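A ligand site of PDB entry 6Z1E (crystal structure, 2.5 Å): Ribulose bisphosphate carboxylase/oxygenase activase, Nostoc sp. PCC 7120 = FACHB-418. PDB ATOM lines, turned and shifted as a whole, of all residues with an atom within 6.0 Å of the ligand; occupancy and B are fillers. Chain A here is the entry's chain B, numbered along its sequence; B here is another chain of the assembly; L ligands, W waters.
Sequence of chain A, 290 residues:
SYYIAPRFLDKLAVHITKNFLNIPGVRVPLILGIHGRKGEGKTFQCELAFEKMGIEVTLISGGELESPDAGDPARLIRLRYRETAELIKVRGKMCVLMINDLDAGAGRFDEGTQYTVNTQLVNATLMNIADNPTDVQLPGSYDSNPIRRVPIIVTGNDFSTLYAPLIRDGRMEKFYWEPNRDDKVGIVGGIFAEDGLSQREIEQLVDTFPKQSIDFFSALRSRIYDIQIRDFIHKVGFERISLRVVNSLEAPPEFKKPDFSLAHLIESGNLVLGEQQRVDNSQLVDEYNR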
ATOM      1  N   TYR A   2     -14.409  -4.613  -3.697  1.00  0.00           N
ATOM      2  CA  TYR A   2     -13.242  -3.938  -4.254  1.00  0.00           C
ATOM      3  C   TYR A   2     -13.199  -2.474  -3.869  1.00  0.00           C
ATOM      4  O   TYR A   2     -14.215  -1.792  -3.827  1.00  0.00           O
ATOM      5  CB  TYR A   2     -13.217  -4.103  -5.774  1.00  0.00           C
ATOM      6  CG  TYR A   2     -12.991  -5.532  -6.215  1.00  0.00           C
ATOM      7  CD1 TYR A   2     -12.025  -6.319  -5.600  1.00  0.00           C
ATOM      8  CD2 TYR A   2     -13.736  -6.085  -7.242  1.00  0.00           C
ATOM      9  CE1 TYR A   2     -11.807  -7.623  -5.992  1.00  0.00           C
ATOM     10  CE2 TYR A   2     -13.533  -7.396  -7.645  1.00  0.00           C
ATOM     11  CZ  TYR A   2     -12.576  -8.159  -7.013  1.00  0.00           C
ATOM     12  OH  TYR A   2     -12.358  -9.463  -7.405  1.00  0.00           O
ATOM     13  N   TYR A   3     -11.985  -2.000  -3.609  1.00  0.00           N
ATOM     14  CA  TYR A   3     -11.758  -0.664  -3.063  1.00  0.00           C
ATOM     15  C   TYR A   3     -11.425   0.339  -4.166  1.00  0.00           C
ATOM     16  O   TYR A   3     -10.568   0.085  -5.018  1.00  0.00           O
ATOM     17  CB  TYR A   3     -10.616  -0.733  -2.053  1.00  0.00           C
ATOM     18  CG  TYR A   3     -10.207   0.583  -1.426  1.00  0.00           C
ATOM     19  CD1 TYR A   3     -10.796   1.031  -0.259  1.00  0.00           C
ATOM     20  CD2 TYR A   3      -9.200   1.353  -1.991  1.00  0.00           C
ATOM     21  CE1 TYR A   3     -10.408   2.226   0.323  1.00  0.00           C
ATOM     22  CE2 TYR A   3      -8.806   2.548  -1.416  1.00  0.00           C
ATOM     23  CZ  TYR A   3      -9.422   2.977  -0.256  1.00  0.00           C
ATOM     24  OH  TYR A   3      -9.028   4.172   0.318  1.00  0.00           O
ATOM     25  N   ILE A   4     -12.125   1.467  -4.143  1.00  0.00           N
ATOM     26  CA  ILE A   4     -11.823   2.600  -5.018  1.00  0.00           C
ATOM     27  C   ILE A   4     -11.111   3.662  -4.175  1.00  0.00           C
ATOM     28  O   ILE A   4     -11.574   4.015  -3.098  1.00  0.00           O
ATOM     29  CB  ILE A   4     -13.101   3.169  -5.683  1.00  0.00           C
ATOM     30  CG1 ILE A   4     -12.784   4.423  -6.504  1.00  0.00           C
ATOM     31  CG2 ILE A   4     -14.170   3.497  -4.642  1.00  0.00           C
ATOM     32  CD1 ILE A   4     -11.901   4.171  -7.693  1.00  0.00           C
ATOM     33  N   GLY A  36       0.225   6.964 -15.742  1.00  0.00           N
ATOM     34  CA  GLY A  36       0.993   6.369 -14.676  1.00  0.00           C
ATOM     35  C   GLY A  36       1.464   4.981 -15.068  1.00  0.00           C
ATOM     36  O   GLY A  36       1.196   4.511 -16.167  1.00  0.00           O
ATOM     37  N   ARG A  37       2.172   4.315 -14.152  1.00  0.00           N
ATOM     38  CA  ARG A  37       2.705   2.990 -14.430  1.00  0.00           C
ATOM     39  C   ARG A  37       1.604   2.019 -14.818  1.00  0.00           C
ATOM     40  O   ARG A  37       0.449   2.170 -14.404  1.00  0.00           O
ATOM     41  CB  ARG A  37       3.462   2.458 -13.216  1.00  0.00           C
ATOM     42  CG  ARG A  37       4.060   1.077 -13.445  1.00  0.00           C
ATOM     43  CD  ARG A  37       5.101   0.717 -12.394  1.00  0.00           C
ATOM     44  NE  ARG A  37       4.550   0.668 -11.041  1.00  0.00           N
ATOM     45  CZ  ARG A  37       5.274   0.372  -9.960  1.00  0.00           C
ATOM     46  NH1 ARG A  37       6.564   0.112 -10.075  1.00  0.00           N
ATOM     47  NH2 ARG A  37       4.705   0.355  -8.768  1.00  0.00           N
ATOM     48  N   LYS A  38       1.961   1.026 -15.618  1.00  0.00           N
ATOM     49  CA  LYS A  38       1.017   0.018 -16.063  1.00  0.00           C
ATOM     50  C   LYS A  38       0.558  -0.844 -14.897  1.00  0.00           C
ATOM     51  O   LYS A  38       1.321  -1.138 -13.985  1.00  0.00           O
ATOM     52  CB  LYS A  38       1.669  -0.858 -17.139  1.00  0.00           C
ATOM     53  CG  LYS A  38       0.809  -2.007 -17.641  1.00  0.00           C
ATOM     54  CD  LYS A  38       1.606  -2.942 -18.537  1.00  0.00           C
ATOM     55  CE  LYS A  38       0.835  -4.211 -18.835  1.00  0.00           C
ATOM     56  NZ  LYS A  38      -0.454  -3.924 -19.518  1.00  0.00           N
ATOM     57  N   GLY A  39      -0.708  -1.249 -14.939  1.00  0.00           N
ATOM     58  CA  GLY A  39      -1.252  -2.164 -13.953  1.00  0.00           C
ATOM     59  C   GLY A  39      -1.321  -1.585 -12.560  1.00  0.00           C
ATOM     60  O   GLY A  39      -1.029  -2.278 -11.581  1.00  0.00           O
ATOM     61  N   GLU A  40      -1.701  -0.314 -12.453  1.00  0.00           N
ATOM     62  CA  GLU A  40      -1.909   0.334 -11.161  1.00  0.00           C
ATOM     63  C   GLU A  40      -3.396   0.556 -10.901  1.00  0.00           C
ATOM     64  O   GLU A  40      -3.770   1.176  -9.910  1.00  0.00           O
ATOM     65  CB  GLU A  40      -1.149   1.655 -11.082  1.00  0.00           C
ATOM     66  CG  GLU A  40       0.372   1.532 -11.225  1.00  0.00           C
ATOM     67  CD  GLU A  40       1.040   0.952  -9.985  1.00  0.00           C
ATOM     68  OE1 GLU A  40       0.352   0.322  -9.165  1.00  0.00           O
ATOM     69  OE2 GLU A  40       2.270   1.127  -9.846  1.00  0.00           O
ATOM     70  N   GLY A  41      -4.243   0.060 -11.795  1.00  0.00           N
ATOM     71  CA  GLY A  41      -5.676   0.120 -11.612  1.00  0.00           C
ATOM     72  C   GLY A  41      -6.346   1.331 -12.222  1.00  0.00           C
ATOM     73  O   GLY A  41      -7.427   1.729 -11.783  1.00  0.00           O
ATOM     74  N   LYS A  42      -5.718   1.937 -13.219  1.00  0.00           N
ATOM     75  CA  LYS A  42      -6.322   3.058 -13.926  1.00  0.00           C
ATOM     76  C   LYS A  42      -7.651   2.642 -14.540  1.00  0.00           C
ATOM     77  O   LYS A  42      -8.670   3.305 -14.351  1.00  0.00           O
ATOM     78  CB  LYS A  42      -5.391   3.617 -15.000  1.00  0.00           C
ATOM     79  CG  LYS A  42      -4.304   4.525 -14.460  1.00  0.00           C
ATOM     80  CD  LYS A  42      -3.265   4.861 -15.519  1.00  0.00           C
ATOM     81  CE  LYS A  42      -2.101   3.884 -15.490  1.00  0.00           C
ATOM     82  NZ  LYS A  42      -1.834   3.262 -16.827  1.00  0.00           N
ATOM     83  N   THR A  43      -7.651   1.523 -15.267  1.00  0.00           N
ATOM     84  CA  THR A  43      -8.877   1.039 -15.878  1.00  0.00           C
ATOM     85  C   THR A  43      -9.838   0.499 -14.827  1.00  0.00           C
ATOM     86  O   THR A  43     -11.028   0.828 -14.841  1.00  0.00           O
ATOM     87  CB  THR A  43      -8.583  -0.069 -16.926  1.00  0.00           C
ATOM     88  OG1 THR A  43      -7.857   0.496 -18.023  1.00  0.00           O
ATOM     89  CG2 THR A  43      -9.885  -0.682 -17.462  1.00  0.00           C
ATOM     90  N   PHE A  44      -9.333  -0.325 -13.912  1.00  0.00           N
ATOM     91  CA  PHE A  44     -10.188  -1.019 -12.961  1.00  0.00           C
ATOM     92  C   PHE A  44     -10.953  -0.053 -12.056  1.00  0.00           C
ATOM     93  O   PHE A  44     -12.121  -0.269 -11.756  1.00  0.00           O
ATOM     94  CB  PHE A  44      -9.356  -1.984 -12.101  1.00  0.00           C
ATOM     95  CG  PHE A  44     -10.176  -3.038 -11.413  1.00  0.00           C
ATOM     96  CD1 PHE A  44     -10.756  -2.784 -10.181  1.00  0.00           C
ATOM     97  CD2 PHE A  44     -10.364  -4.278 -11.999  1.00  0.00           C
ATOM     98  CE1 PHE A  44     -11.510  -3.749  -9.550  1.00  0.00           C
ATOM     99  CE2 PHE A  44     -11.118  -5.243 -11.367  1.00  0.00           C
ATOM    100  CZ  PHE A  44     -11.687  -4.977 -10.140  1.00  0.00           C
ATOM    101  N   GLN A  45     -10.274   1.011 -11.629  1.00  0.00           N
ATOM    102  CA  GLN A  45     -10.901   1.996 -10.750  1.00  0.00           C
ATOM    103  C   GLN A  45     -11.850   2.926 -11.494  1.00  0.00           C
ATOM    104  O   GLN A  45     -12.797   3.453 -10.917  1.00  0.00           O
ATOM    105  CB  GLN A  45      -9.834   2.841 -10.049  1.00  0.00           C
ATOM    106  CG  GLN A  45      -9.130   2.103  -8.935  1.00  0.00           C
ATOM    107  CD  GLN A  45      -8.124   2.984  -8.243  1.00  0.00           C
ATOM    108  OE1 GLN A  45      -8.272   3.303  -7.063  1.00  0.00           O
ATOM    109  NE2 GLN A  45      -7.108   3.399  -8.980  1.00  0.00           N
ATOM    110  N   LEU A  48     -14.933   0.929 -11.443  1.00  0.00           N
ATOM    111  CA  LEU A  48     -15.551   0.949 -10.128  1.00  0.00           C
ATOM    112  C   LEU A  48     -16.364   2.225  -9.935  1.00  0.00           C
ATOM    113  O   LEU A  48     -17.461   2.201  -9.387  1.00  0.00           O
ATOM    114  CB  LEU A  48     -14.492   0.806  -9.027  1.00  0.00           C
ATOM    115  CG  LEU A  48     -13.862  -0.591  -8.901  1.00  0.00           C
ATOM    116  CD1 LEU A  48     -12.752  -0.576  -7.858  1.00  0.00           C
ATOM    117  CD2 LEU A  48     -14.899  -1.666  -8.575  1.00  0.00           C
ATOM    118  N   ASN A 100      -8.785   3.225 -23.679  1.00  0.00           N
ATOM    119  CA  ASN A 100      -7.892   2.508 -22.776  1.00  0.00           C
ATOM    120  C   ASN A 100      -6.512   2.238 -23.354  1.00  0.00           C
ATOM    121  O   ASN A 100      -6.381   1.953 -24.547  1.00  0.00           O
ATOM    122  CB  ASN A 100      -8.544   1.166 -22.421  1.00  0.00           C
ATOM    123  CG  ASN A 100      -8.765   0.998 -20.937  1.00  0.00           C
ATOM    124  OD1 ASN A 100      -9.768   0.429 -20.516  1.00  0.00           O
ATOM    125  ND2 ASN A 100      -7.833   1.495 -20.130  1.00  0.00           N
ATOM    126  N   ASP A 101      -5.493   2.292 -22.500  1.00  0.00           N
ATOM    127  CA  ASP A 101      -4.146   1.863 -22.860  1.00  0.00           C
ATOM    128  C   ASP A 101      -3.657   2.563 -24.120  1.00  0.00           C
ATOM    129  O   ASP A 101      -3.193   1.914 -25.058  1.00  0.00           O
ATOM    130  CB  ASP A 101      -4.126   0.352 -23.063  1.00  0.00           C
ATOM    131  CG  ASP A 101      -4.757  -0.409 -21.913  1.00  0.00           C
ATOM    132  OD1 ASP A 101      -4.777   0.130 -20.790  1.00  0.00           O
ATOM    133  OD2 ASP A 101      -5.232  -1.545 -22.143  1.00  0.00           O
ATOM    134  N   THR A 155      -6.722   6.678 -20.884  1.00  0.00           N
ATOM    135  CA  THR A 155      -5.803   5.949 -20.012  1.00  0.00           C
ATOM    136  C   THR A 155      -4.576   5.588 -20.816  1.00  0.00           C
ATOM    137  O   THR A 155      -4.678   5.208 -21.986  1.00  0.00           O
ATOM    138  CB  THR A 155      -6.473   4.669 -19.464  1.00  0.00           C
ATOM    139  OG1 THR A 155      -7.269   4.997 -18.315  1.00  0.00           O
ATOM    140  CG2 THR A 155      -5.444   3.604 -19.072  1.00  0.00           C
ATOM    141  N   ASN A 157       0.175   5.022 -20.339  1.00  0.00           N
ATOM    142  CA  ASN A 157       1.340   5.064 -19.467  1.00  0.00           C
ATOM    143  C   ASN A 157       1.845   6.490 -19.341  1.00  0.00           C
ATOM    144  O   ASN A 157       2.086   6.986 -18.238  1.00  0.00           O
ATOM    145  CB  ASN A 157       2.429   4.137 -20.009  1.00  0.00           C
ATOM    146  CG  ASN A 157       1.989   2.694 -20.051  1.00  0.00           C
ATOM    147  OD1 ASN A 157       0.978   2.316 -19.435  1.00  0.00           O
ATOM    148  ND2 ASN A 157       2.735   1.862 -20.767  1.00  0.00           N
ATOM    149  N   TRP A 177      -1.468   8.979 -11.843  1.00  0.00           N
ATOM    150  CA  TRP A 177      -1.927   7.999 -10.867  1.00  0.00           C
ATOM    151  C   TRP A 177      -0.788   7.113 -10.370  1.00  0.00           C
ATOM    152  O   TRP A 177      -0.294   6.247 -11.091  1.00  0.00           O
ATOM    153  CB  TRP A 177      -3.028   7.121 -11.443  1.00  0.00           C
ATOM    154  CG  TRP A 177      -3.412   6.037 -10.494  1.00  0.00           C
ATOM    155  CD1 TRP A 177      -3.335   4.695 -10.714  1.00  0.00           C
ATOM    156  CD2 TRP A 177      -3.901   6.202  -9.156  1.00  0.00           C
ATOM    157  NE1 TRP A 177      -3.760   4.011  -9.594  1.00  0.00           N
ATOM    158  CE2 TRP A 177      -4.109   4.918  -8.624  1.00  0.00           C
ATOM    159  CE3 TRP A 177      -4.189   7.316  -8.362  1.00  0.00           C
ATOM    160  CZ2 TRP A 177      -4.590   4.713  -7.335  1.00  0.00           C
ATOM    161  CZ3 TRP A 177      -4.659   7.110  -7.089  1.00  0.00           C
ATOM    162  CH2 TRP A 177      -4.855   5.813  -6.585  1.00  0.00           C
ATOM    163  N   ILE A 187      -6.797  -1.200  -1.678  1.00  0.00           N
ATOM    164  CA  ILE A 187      -6.955  -2.009  -2.902  1.00  0.00           C
ATOM    165  C   ILE A 187      -6.546  -3.467  -2.660  1.00  0.00           C
ATOM    166  O   ILE A 187      -7.292  -4.384  -3.019  1.00  0.00           O
ATOM    167  CB  ILE A 187      -6.139  -1.417  -4.071  1.00  0.00           C
ATOM    168  CG1 ILE A 187      -6.655  -0.025  -4.435  1.00  0.00           C
ATOM    169  CG2 ILE A 187      -6.228  -2.316  -5.303  1.00  0.00           C
ATOM    170  CD1 ILE A 187      -5.675   0.796  -5.254  1.00  0.00           C
ATOM    171  N   GLY A 190      -8.967  -5.376  -0.622  1.00  0.00           N
ATOM    172  CA  GLY A 190     -10.137  -5.803  -1.368  1.00  0.00           C
ATOM    173  C   GLY A 190      -9.856  -7.003  -2.249  1.00  0.00           C
ATOM    174  O   GLY A 190     -10.765  -7.773  -2.572  1.00  0.00           O
ATOM    175  N   ILE A 191      -8.599  -7.165  -2.638  1.00  0.00           N
ATOM    176  CA  ILE A 191      -8.174  -8.311  -3.443  1.00  0.00           C
ATOM    177  C   ILE A 191      -8.201  -9.592  -2.599  1.00  0.00           C
ATOM    178  O   ILE A 191      -8.591 -10.651  -3.092  1.00  0.00           O
ATOM    179  CB  ILE A 191      -6.771  -8.104  -4.042  1.00  0.00           C
ATOM    180  CG1 ILE A 191      -6.806  -6.968  -5.082  1.00  0.00           C
ATOM    181  CG2 ILE A 191      -6.244  -9.380  -4.695  1.00  0.00           C
ATOM    182  CD1 ILE A 191      -5.436  -6.506  -5.545  1.00  0.00           C
ATOM    183  N   ILE A 214      -0.151  -2.746  -8.346  1.00  0.00           N
ATOM    184  CA  ILE A 214      -1.340  -3.463  -7.901  1.00  0.00           C
ATOM    185  C   ILE A 214      -1.469  -4.771  -8.662  1.00  0.00           C
ATOM    186  O   ILE A 214      -1.959  -5.767  -8.136  1.00  0.00           O
ATOM    187  CB  ILE A 214      -2.620  -2.600  -8.068  1.00  0.00           C
ATOM    188  CG1 ILE A 214      -2.752  -1.608  -6.924  1.00  0.00           C
ATOM    189  CG2 ILE A 214      -3.874  -3.459  -8.078  1.00  0.00           C
ATOM    190  CD1 ILE A 214      -1.777  -0.477  -6.989  1.00  0.00           C
ATOM    191  N   ASP A 215      -1.004  -4.773  -9.915  1.00  0.00           N
ATOM    192  CA  ASP A 215      -1.046  -5.954 -10.767  1.00  0.00           C
ATOM    193  C   ASP A 215      -0.280  -7.129 -10.152  1.00  0.00           C
ATOM    194  O   ASP A 215      -0.700  -8.277 -10.268  1.00  0.00           O
ATOM    195  CB  ASP A 215      -0.454  -5.624 -12.143  1.00  0.00           C
ATOM    196  CG  ASP A 215      -0.686  -6.722 -13.160  1.00  0.00           C
ATOM    197  OD1 ASP A 215      -1.803  -7.296 -13.186  1.00  0.00           O
ATOM    198  OD2 ASP A 215       0.238  -7.015 -13.937  1.00  0.00           O
ATOM    199  N   SER A 218      -2.587  -8.881  -7.330  1.00  0.00           N
ATOM    200  CA  SER A 218      -3.670  -9.703  -7.871  1.00  0.00           C
ATOM    201  C   SER A 218      -3.085 -10.940  -8.559  1.00  0.00           C
ATOM    202  O   SER A 218      -3.712 -11.992  -8.581  1.00  0.00           O
ATOM    203  CB  SER A 218      -4.530  -8.901  -8.854  1.00  0.00           C
ATOM    204  OG  SER A 218      -3.738  -8.334  -9.879  1.00  0.00           O
ATOM    205  N   ARG B 168      -7.067  -8.581 -18.778  1.00  0.00           N
ATOM    206  CA  ARG B 168      -7.626  -7.814 -17.679  1.00  0.00           C
ATOM    207  C   ARG B 168      -8.786  -8.541 -16.992  1.00  0.00           C
ATOM    208  O   ARG B 168      -9.002  -8.371 -15.792  1.00  0.00           O
ATOM    209  CB  ARG B 168      -8.095  -6.444 -18.192  1.00  0.00           C
ATOM    210  CG  ARG B 168      -8.138  -5.365 -17.137  1.00  0.00           C
ATOM    211  CD  ARG B 168      -8.560  -4.044 -17.725  1.00  0.00           C
ATOM    212  NE  ARG B 168      -7.445  -3.103 -17.805  1.00  0.00           N
ATOM    213  CZ  ARG B 168      -6.781  -2.790 -18.920  1.00  0.00           C
ATOM    214  NH1 ARG B 168      -7.103  -3.322 -20.091  1.00  0.00           N
ATOM    215  NH2 ARG B 168      -5.787  -1.911 -18.862  1.00  0.00           N
HETATM  216  P1  LIG L   1      -3.797  -0.013 -15.941  1.00  0.00           P
HETATM  217  O1  LIG L   1      -5.098   0.255 -16.558  1.00  0.00           O
HETATM  218  O2  LIG L   1      -3.219   0.994 -15.056  1.00  0.00           O
HETATM  219  O3  LIG L   1      -2.863  -0.941 -16.593  1.00  0.00           O
HETATM  220  P2  LIG L   1      -5.411  -2.053 -14.626  1.00  0.00           P
HETATM  221  O4  LIG L   1      -5.379  -2.758 -15.928  1.00  0.00           O
HETATM  222  O5  LIG L   1      -6.701  -1.557 -14.130  1.00  0.00           O
HETATM  223  O6  LIG L   1      -4.320  -0.870 -14.685  1.00  0.00           O
HETATM  224  O7  LIG L   1      -4.700  -3.055 -13.567  1.00  0.00           O
HETATM  225  C1  LIG L   1      -4.437  -4.445 -13.788  1.00  0.00           C
HETATM  226  C2  LIG L   1      -5.434  -5.037 -12.784  1.00  0.00           C
HETATM  227  O8  LIG L   1      -4.717  -5.254 -11.442  1.00  0.00           O
HETATM  228  C3  LIG L   1      -6.881  -4.919 -12.466  1.00  0.00           C
HETATM  229  O9  LIG L   1      -7.617  -5.495 -13.510  1.00  0.00           O
HETATM  230  C4  LIG L   1      -6.605  -6.076 -11.279  1.00  0.00           C
HETATM  231  O10 LIG L   1      -6.382  -7.481 -11.748  1.00  0.00           O
HETATM  232  C5  LIG L   1      -5.592  -5.612 -10.290  1.00  0.00           C
HETATM  233  N1  LIG L   1      -6.482  -4.447  -9.900  1.00  0.00           N
HETATM  234  C6  LIG L   1      -6.270  -3.148 -10.185  1.00  0.00           C
HETATM  235  N2  LIG L   1      -7.155  -2.403  -9.513  1.00  0.00           N
HETATM  236  C7  LIG L   1      -7.843  -3.195  -8.709  1.00  0.00           C
HETATM  237  C8  LIG L   1      -8.814  -2.932  -7.828  1.00  0.00           C
HETATM  238  N3  LIG L   1      -9.204  -1.656  -7.691  1.00  0.00           N
HETATM  239  N4  LIG L   1      -9.396  -3.884  -7.100  1.00  0.00           N
HETATM  240  C9  LIG L   1      -8.954  -5.196  -7.272  1.00  0.00           C
HETATM  241  N5  LIG L   1      -7.927  -5.457  -8.199  1.00  0.00           N
HETATM  242  C10 LIG L   1      -7.388  -4.446  -8.899  1.00  0.00           C
HETATM  243  O   HOH W   1      -9.862  -3.716  -4.212  1.00  0.00           O
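N of Gly 39 lies within hydrogen-bond range of O3 of the ligand (2.7 Å). An oxygen (O4) of the ligand is in salt-bridge range of the guanidinium group (NE) of Arg 168 of chain B, at 2.8 Å. N of Phe 44 sits at hydrogen-bond distance from O5 of the ligand (2.9 Å). The backbone NH (N) of Gly 41 sits at hydrogen-bond distance from an oxygen (O6) of the ligand (3.0 Å). N of Thr 43 is in hydrogen-bond range of O1 of the ligand, 3.1 Å away. The side-chain hydroxyl (OG1) of Thr 43 is in hydrogen-bond range of an oxygen (O1) of the ligand. O2 of the ligand lies close to N of Lys 42, 3.2 Å away. An oxygen (O2) of the ligand is in salt-bridge range of the side-chain amino group (NZ) of Lys 42, at 3.2 Å. O2 of the ligand sits at hydrogen-bond distance from N of Glu 40, at 3.3 Å. OG of Ser 218 sits close to O10 of the ligand. A nitrogen (N3) of the ligand sits at hydrogen-bond distance from the backbone carbonyl oxygen (O) of Tyr 3, at 3.5 Å.
The backbone carbonyl oxygen (O) of Gly 39 lies within hydrogen-bond range of the backbone NH (N) of Ile 214 (3.4 Å). OG1 of Thr 43 is in hydrogen-bond range of NH2 of Arg 168 of chain B, 3.3 Å away. The backbone carbonyl oxygen (O) of Gly 41 sits close to the side-chain amide nitrogen (NE2) of Gln 45 (3.3 Å). The backbone NH (N) of Ile 214 lies close to the side-chain carboxylate (OE1) of Glu 40, 3.2 Å away. NE of Arg 37 is in salt-bridge range of OE2 of Glu 40 (2.6 Å). O of Glu 40 sits at hydrogen-bond distance from NE1 of Trp 177 (2.9 Å). OG of Ser 218 is in hydrogen-bond range of O of Asp 215, at 3.1 Å. The side-chain amide nitrogen (NE2) of Gln 45 sits close to the indole nitrogen (NE1) of Trp 177, 3.5 Å away.
Residues that only touch the ligand: Ile 214 (3.2 Å), Ile 191 (3.5 Å), Ile 187 (3.7 Å), Tyr 2 (3.7 Å), Leu 48 (3.7 Å), Asp 215 (3.8 Å), Lys 38 (3.8 Å), Arg 37 (3.9 Å) and Gln 45 (3.96 Å). Hydrophobic or aromatic side chains that line the ligand: Tyr 2, Phe 44, Leu 48, Ile 187, Ile 191 and Ile 214. The nearest printed residue that does not touch the ligand is Thr 155 (4.2 Å).
Water W1 lies within hydrogen-bond range of the backbone NH of Tyr 3 (2.8 Å), the backbone carbonyl oxygen of Ile 187 (2.9 Å) and a nitrogen (N4) of the ligand (2.9 Å).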
